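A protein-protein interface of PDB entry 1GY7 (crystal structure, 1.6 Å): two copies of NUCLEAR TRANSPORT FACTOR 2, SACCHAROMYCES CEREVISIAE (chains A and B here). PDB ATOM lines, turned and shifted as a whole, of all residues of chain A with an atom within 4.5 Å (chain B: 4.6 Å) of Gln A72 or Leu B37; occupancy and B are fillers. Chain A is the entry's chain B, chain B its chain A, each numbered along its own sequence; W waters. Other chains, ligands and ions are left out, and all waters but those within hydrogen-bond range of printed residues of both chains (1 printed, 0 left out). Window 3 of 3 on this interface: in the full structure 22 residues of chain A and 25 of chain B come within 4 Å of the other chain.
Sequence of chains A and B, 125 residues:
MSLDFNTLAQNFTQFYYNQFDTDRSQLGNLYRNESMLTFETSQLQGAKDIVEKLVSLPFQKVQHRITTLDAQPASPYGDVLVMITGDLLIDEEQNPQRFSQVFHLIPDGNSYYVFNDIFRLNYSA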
ATOM      1  N   PHE A   5     -11.093  27.456 -17.911  1.00  0.00           N
ATOM      2  CA  PHE A   5     -10.488  27.248 -19.217  1.00  0.00           C
ATOM      3  C   PHE A   5     -10.977  28.301 -20.197  1.00  0.00           C
ATOM      4  O   PHE A   5     -10.254  28.677 -21.117  1.00  0.00           O
ATOM      5  CB  PHE A   5     -10.798  25.846 -19.747  1.00  0.00           C
ATOM      6  CG  PHE A   5     -10.036  24.764 -19.048  1.00  0.00           C
ATOM      7  CD1 PHE A   5     -10.583  24.103 -17.953  1.00  0.00           C
ATOM      8  CD2 PHE A   5      -8.748  24.436 -19.456  1.00  0.00           C
ATOM      9  CE1 PHE A   5      -9.853  23.131 -17.272  1.00  0.00           C
ATOM     10  CE2 PHE A   5      -8.011  23.468 -18.784  1.00  0.00           C
ATOM     11  CZ  PHE A   5      -8.565  22.813 -17.688  1.00  0.00           C
ATOM     12  N   ALA A  71     -14.236  26.791 -24.184  1.00  0.00           N
ATOM     13  CA  ALA A  71     -13.012  26.005 -24.135  1.00  0.00           C
ATOM     14  C   ALA A  71     -13.099  24.815 -23.200  1.00  0.00           C
ATOM     15  O   ALA A  71     -13.907  24.792 -22.267  1.00  0.00           O
ATOM     16  CB  ALA A  71     -11.852  26.885 -23.723  1.00  0.00           C
ATOM     17  N   GLN A  72     -12.250  23.831 -23.467  1.00  0.00           N
ATOM     18  CA  GLN A  72     -12.159  22.627 -22.652  1.00  0.00           C
ATOM     19  C   GLN A  72     -10.717  22.150 -22.672  1.00  0.00           C
ATOM     20  O   GLN A  72      -9.962  22.454 -23.594  1.00  0.00           O
ATOM     21  CB  GLN A  72     -12.996  21.483 -23.237  1.00  0.00           C
ATOM     22  CG  GLN A  72     -14.490  21.693 -23.313  1.00  0.00           C
ATOM     23  CD  GLN A  72     -15.202  20.449 -23.831  1.00  0.00           C
ATOM     24  OE1 GLN A  72     -14.563  19.535 -24.366  1.00  0.00           O
ATOM     25  NE2 GLN A  72     -16.525  20.413 -23.692  1.00  0.00           N
ATOM     26  N   PRO A  73     -10.303  21.414 -21.639  1.00  0.00           N
ATOM     27  CA  PRO A  73      -8.926  20.917 -21.660  1.00  0.00           C
ATOM     28  C   PRO A  73      -8.922  19.871 -22.791  1.00  0.00           C
ATOM     29  O   PRO A  73      -9.819  19.019 -22.854  1.00  0.00           O
ATOM     30  CB  PRO A  73      -8.757  20.294 -20.274  1.00  0.00           C
ATOM     31  CG  PRO A  73     -10.171  19.977 -19.839  1.00  0.00           C
ATOM     32  CD  PRO A  73     -10.956  21.156 -20.344  1.00  0.00           C
ATOM     33  N   ALA A  74      -7.939  19.941 -23.683  1.00  0.00           N
ATOM     34  CA  ALA A  74      -7.872  19.017 -24.821  1.00  0.00           C
ATOM     35  C   ALA A  74      -7.377  17.629 -24.448  1.00  0.00           C
ATOM     36  O   ALA A  74      -7.528  16.672 -25.210  1.00  0.00           O
ATOM     37  CB  ALA A  74      -6.999  19.607 -25.911  1.00  0.00           C
ATOM     38  N   VAL A  80      -5.228  23.034 -24.506  1.00  0.00           N
ATOM     39  CA  VAL A  80      -6.593  23.523 -24.477  1.00  0.00           C
ATOM     40  C   VAL A  80      -7.234  23.546 -25.852  1.00  0.00           C
ATOM     41  O   VAL A  80      -6.573  23.799 -26.858  1.00  0.00           O
ATOM     42  CB  VAL A  80      -6.624  24.959 -23.888  1.00  0.00           C
ATOM     43  CG1 VAL A  80      -8.050  25.478 -23.830  1.00  0.00           C
ATOM     44  CG2 VAL A  80      -5.986  24.966 -22.500  1.00  0.00           C
ATOM     45  N   LEU A  81      -8.528  23.267 -25.883  1.00  0.00           N
ATOM     46  CA  LEU A  81      -9.290  23.289 -27.121  1.00  0.00           C
ATOM     47  C   LEU A  81     -10.283  24.433 -26.973  1.00  0.00           C
ATOM     48  O   LEU A  81     -10.976  24.531 -25.957  1.00  0.00           O
ATOM     49  CB  LEU A  81     -10.049  21.981 -27.296  1.00  0.00           C
ATOM     50  CG  LEU A  81     -10.872  21.882 -28.576  1.00  0.00           C
ATOM     51  CD1 LEU A  81      -9.924  21.785 -29.763  1.00  0.00           C
ATOM     52  CD2 LEU A  81     -11.780  20.662 -28.507  1.00  0.00           C
ATOM     53  N   SER B  35     -14.913  11.982 -20.921  1.00  0.00           N
ATOM     54  CA  SER B  35     -15.499  12.867 -21.923  1.00  0.00           C
ATOM     55  C   SER B  35     -16.177  14.119 -21.391  1.00  0.00           C
ATOM     56  O   SER B  35     -16.814  14.101 -20.343  1.00  0.00           O
ATOM     57  CB  SER B  35     -16.495  12.087 -22.782  1.00  0.00           C
ATOM     58  OG  SER B  35     -15.852  11.017 -23.446  1.00  0.00           O
ATOM     59  N   MET B  36     -16.039  15.213 -22.132  1.00  0.00           N
ATOM     60  CA  MET B  36     -16.654  16.473 -21.735  1.00  0.00           C
ATOM     61  C   MET B  36     -17.516  17.045 -22.838  1.00  0.00           C
ATOM     62  O   MET B  36     -17.121  17.061 -24.008  1.00  0.00           O
ATOM     63  CB  MET B  36     -15.589  17.499 -21.380  1.00  0.00           C
ATOM     64  CG  MET B  36     -14.737  17.099 -20.204  1.00  0.00           C
ATOM     65  SD  MET B  36     -13.226  18.051 -20.175  1.00  0.00           S
ATOM     66  CE  MET B  36     -12.225  17.064 -21.267  1.00  0.00           C
ATOM     67  N   LEU B  37     -18.699  17.508 -22.451  1.00  0.00           N
ATOM     68  CA  LEU B  37     -19.629  18.128 -23.381  1.00  0.00           C
ATOM     69  C   LEU B  37     -19.951  19.540 -22.926  1.00  0.00           C
ATOM     70  O   LEU B  37     -20.325  19.761 -21.774  1.00  0.00           O
ATOM     71  CB  LEU B  37     -20.955  17.349 -23.463  1.00  0.00           C
ATOM     72  CG  LEU B  37     -22.104  18.133 -24.138  1.00  0.00           C
ATOM     73  CD1 LEU B  37     -21.774  18.380 -25.603  1.00  0.00           C
ATOM     74  CD2 LEU B  37     -23.419  17.379 -24.015  1.00  0.00           C
ATOM     75  N   THR B  38     -19.771  20.500 -23.820  1.00  0.00           N
ATOM     76  CA  THR B  38     -20.158  21.864 -23.516  1.00  0.00           C
ATOM     77  C   THR B  38     -21.293  22.078 -24.492  1.00  0.00           C
ATOM     78  O   THR B  38     -21.072  22.220 -25.694  1.00  0.00           O
ATOM     79  CB  THR B  38     -19.050  22.893 -23.792  1.00  0.00           C
ATOM     80  OG1 THR B  38     -17.985  22.710 -22.852  1.00  0.00           O
ATOM     81  CG2 THR B  38     -19.604  24.313 -23.641  1.00  0.00           C
ATOM     82  N   PHE B  39     -22.516  22.029 -23.983  1.00  0.00           N
ATOM     83  CA  PHE B  39     -23.676  22.227 -24.828  1.00  0.00           C
ATOM     84  C   PHE B  39     -24.153  23.626 -24.495  1.00  0.00           C
ATOM     85  O   PHE B  39     -24.897  23.828 -23.536  1.00  0.00           O
ATOM     86  CB  PHE B  39     -24.756  21.200 -24.507  1.00  0.00           C
ATOM     87  CG  PHE B  39     -25.892  21.200 -25.488  1.00  0.00           C
ATOM     88  CD1 PHE B  39     -25.906  20.307 -26.554  1.00  0.00           C
ATOM     89  CD2 PHE B  39     -26.931  22.119 -25.365  1.00  0.00           C
ATOM     90  CE1 PHE B  39     -26.941  20.328 -27.490  1.00  0.00           C
ATOM     91  CE2 PHE B  39     -27.968  22.149 -26.294  1.00  0.00           C
ATOM     92  CZ  PHE B  39     -27.971  21.250 -27.360  1.00  0.00           C
ATOM     93  N   SER B  42     -24.399  24.599 -20.880  1.00  0.00           N
ATOM     94  CA  SER B  42     -24.376  23.403 -20.037  1.00  0.00           C
ATOM     95  C   SER B  42     -23.042  22.662 -20.141  1.00  0.00           C
ATOM     96  O   SER B  42     -22.571  22.367 -21.237  1.00  0.00           O
ATOM     97  CB  SER B  42     -25.514  22.456 -20.433  1.00  0.00           C
ATOM     98  OG  SER B  42     -26.781  23.075 -20.283  1.00  0.00           O
ATOM     99  N   GLN B  43     -22.435  22.363 -18.997  1.00  0.00           N
ATOM    100  CA  GLN B  43     -21.161  21.647 -18.969  1.00  0.00           C
ATOM    101  C   GLN B  43     -21.328  20.287 -18.289  1.00  0.00           C
ATOM    102  O   GLN B  43     -21.667  20.215 -17.106  1.00  0.00           O
ATOM    103  CB  GLN B  43     -20.107  22.486 -18.241  1.00  0.00           C
ATOM    104  CG  GLN B  43     -19.613  23.685 -19.049  1.00  0.00           C
ATOM    105  CD  GLN B  43     -18.757  24.638 -18.234  1.00  0.00           C
ATOM    106  OE1 GLN B  43     -17.787  24.231 -17.592  1.00  0.00           O
ATOM    107  NE2 GLN B  43     -19.111  25.917 -18.262  1.00  0.00           N
ATOM    108  N   LEU B  44     -21.090  19.211 -19.040  1.00  0.00           N
ATOM    109  CA  LEU B  44     -21.235  17.853 -18.512  1.00  0.00           C
ATOM    110  C   LEU B  44     -19.990  16.994 -18.716  1.00  0.00           C
ATOM    111  O   LEU B  44     -19.220  17.215 -19.648  1.00  0.00           O
ATOM    112  CB  LEU B  44     -22.426  17.145 -19.172  1.00  0.00           C
ATOM    113  CG  LEU B  44     -23.834  17.743 -19.067  1.00  0.00           C
ATOM    114  CD1 LEU B  44     -24.130  18.093 -17.614  1.00  0.00           C
ATOM    115  CD2 LEU B  44     -23.939  18.974 -19.954  1.00  0.00           C
ATOM    116  N   ILE B  50     -23.700  13.268 -20.069  1.00  0.00           N
ATOM    117  CA  ILE B  50     -23.718  13.800 -21.428  1.00  0.00           C
ATOM    118  C   ILE B  50     -24.981  13.350 -22.152  1.00  0.00           C
ATOM    119  O   ILE B  50     -25.713  14.171 -22.701  1.00  0.00           O
ATOM    120  CB  ILE B  50     -22.468  13.347 -22.218  1.00  0.00           C
ATOM    121  CG1 ILE B  50     -21.231  14.052 -21.648  1.00  0.00           C
ATOM    122  CG2 ILE B  50     -22.648  13.632 -23.710  1.00  0.00           C
ATOM    123  CD1 ILE B  50     -19.906  13.619 -22.274  1.00  0.00           C
ATOM    124  N   LYS B  53     -28.158  14.976 -20.877  1.00  0.00           N
ATOM    125  CA  LYS B  53     -28.374  16.321 -21.398  1.00  0.00           C
ATOM    126  C   LYS B  53     -28.973  16.283 -22.802  1.00  0.00           C
ATOM    127  O   LYS B  53     -29.927  17.003 -23.101  1.00  0.00           O
ATOM    128  CB  LYS B  53     -27.054  17.100 -21.418  1.00  0.00           C
ATOM    129  CG  LYS B  53     -27.141  18.458 -22.115  1.00  0.00           C
ATOM    130  CD  LYS B  53     -28.150  19.379 -21.450  1.00  0.00           C
ATOM    131  CE  LYS B  53     -28.254  20.700 -22.207  1.00  0.00           C
ATOM    132  NZ  LYS B  53     -29.193  21.668 -21.575  1.00  0.00           N
ATOM    133  N   LEU B  54     -28.416  15.444 -23.667  1.00  0.00           N
ATOM    134  CA  LEU B  54     -28.926  15.350 -25.028  1.00  0.00           C
ATOM    135  C   LEU B  54     -30.359  14.828 -25.054  1.00  0.00           C
ATOM    136  O   LEU B  54     -31.181  15.300 -25.831  1.00  0.00           O
ATOM    137  CB  LEU B  54     -28.015  14.459 -25.880  1.00  0.00           C
ATOM    138  CG  LEU B  54     -26.567  14.952 -25.959  1.00  0.00           C
ATOM    139  CD1 LEU B  54     -25.766  14.040 -26.873  1.00  0.00           C
ATOM    140  CD2 LEU B  54     -26.531  16.388 -26.480  1.00  0.00           C
ATOM    141  N   ASN B 116     -13.628  15.440 -26.432  1.00  0.00           N
ATOM    142  CA  ASN B 116     -14.144  16.808 -26.316  1.00  0.00           C
ATOM    143  C   ASN B 116     -15.297  16.967 -27.292  1.00  0.00           C
ATOM    144  O   ASN B 116     -15.201  16.551 -28.445  1.00  0.00           O
ATOM    145  CB  ASN B 116     -13.110  17.870 -26.703  1.00  0.00           C
ATOM    146  CG  ASN B 116     -11.922  17.909 -25.783  1.00  0.00           C
ATOM    147  OD1 ASN B 116     -12.026  18.278 -24.608  1.00  0.00           O
ATOM    148  ND2 ASN B 116     -10.774  17.546 -26.313  1.00  0.00           N
ATOM    149  N   ASP B 117     -16.372  17.584 -26.822  1.00  0.00           N
ATOM    150  CA  ASP B 117     -17.542  17.862 -27.641  1.00  0.00           C
ATOM    151  C   ASP B 117     -17.987  19.258 -27.220  1.00  0.00           C
ATOM    152  O   ASP B 117     -18.405  19.458 -26.077  1.00  0.00           O
ATOM    153  CB  ASP B 117     -18.658  16.852 -27.356  1.00  0.00           C
ATOM    154  CG  ASP B 117     -19.912  17.114 -28.172  1.00  0.00           C
ATOM    155  OD1 ASP B 117     -19.988  18.174 -28.830  1.00  0.00           O
ATOM    156  OD2 ASP B 117     -20.831  16.262 -28.153  1.00  0.00           O
ATOM    157  N   ILE B 118     -17.837  20.230 -28.118  1.00  0.00           N
ATOM    158  CA  ILE B 118     -18.259  21.600 -27.839  1.00  0.00           C
ATOM    159  C   ILE B 118     -19.299  21.949 -28.894  1.00  0.00           C
ATOM    160  O   ILE B 118     -19.030  21.855 -30.091  1.00  0.00           O
ATOM    161  CB  ILE B 118     -17.087  22.592 -27.923  1.00  0.00           C
ATOM    162  CG1 ILE B 118     -16.000  22.184 -26.919  1.00  0.00           C
ATOM    163  CG2 ILE B 118     -17.588  24.011 -27.619  1.00  0.00           C
ATOM    164  CD1 ILE B 118     -14.706  22.981 -27.026  1.00  0.00           C
HETATM  165  O   HOH W   1     -16.626  25.005 -22.488  1.00  0.00           O
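Of the 7 printed residues of chain A, 4 touch a printed residue of chain B.
Hydrophobic or aromatic side chains of chain A within 4 Å of the printed part of chain B: Pro A73 and Leu A81.
Hydrophobic or aromatic side chains of chain B that line the printed part of chain A: Met B36 and Ile B118.
Among the printed residues, no Asp or Glu carboxylate lies within 4 Å of a Lys or Arg side-chain nitrogen of the other chain.
Water W1 bridges the side-chain hydroxyl (OG1) of Thr B38 (2.7 Å) and the backbone carbonyl oxygen (O) of Ala A71 (2.7 Å).
Of the printed residues of chain B, Gln A72 touches Met B36, Leu B37, Thr B38, Asn B116, Asp B117 and Ile B118.
Of the printed residues of chain B, Pro A73 touches Met B36 (3.5 Å) and Asn B116 (2.9 Å).
Of the printed residues of chain B, Leu A81 touches Asn B116.
Leu B37 touches just one residue of chain A: Gln A72 (3.6 Å).
Of the printed residues of chain A, Thr B38 touches Gln A72 (2.8 Å).
Printed residues of chain A within 4 Å of Asp B117: Gln A72 (3.2 Å).
Of the printed residues of chain A, Ile B118 touches Gln A72 (3.6 Å).
The nearest printed residue of chain A that does not touch Leu B37 is Ala A71 (8.0 Å).
The nearest printed residue of chain A that does not touch Met B36 is Ala A74 (5.7 Å).
O of Met B36 lies within hydrogen-bond range of N of Asp B117 (3.0 Å).
The backbone NH (N) of Leu B37 sits at hydrogen-bond distance from the backbone carbonyl oxygen (O) of Leu B44 (2.9 Å).
The backbone NH (N) of Thr B38 is in hydrogen-bond range of the backbone carbonyl oxygen (O) of Asp B117.
O of Gln A72 sits at hydrogen-bond distance from N of Leu A81 (2.8 Å).
No position is printed for both chains.
Gln A72 touches Leu B37 (NE2 to C, 3.6 Å).
CD of Gln A72 touches CG1 of Ile B118, at 3.6 Å.
Pro A73 touches Met B36 (O to CE, 3.5 Å).
Ala A74 touches Asn B116 (O to ND2, 3.5 Å).
CD2 of Leu A81 touches CB of Asn B116, at 3.6 Å.
The backbone carbonyl oxygen (O) of Met B36 sits at hydrogen-bond distance from the side-chain amide nitrogen (NE2) of Gln A72.
The side-chain hydroxyl of Thr B38 lies within hydrogen-bond range of the side-chain amide nitrogen of Gln A72 (2.8 Å).
OD1 of Asn B116 lies close to OE1 of Gln A72.
The backbone carbonyl oxygen (O) of Pro A73 lies close to the side-chain amide oxygen (OD1) of Asn B116 (2.9 Å).
The backbone carbonyl oxygen (O) of Asp B117 lies within hydrogen-bond range of the side-chain amide nitrogen (NE2) of Gln A72.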
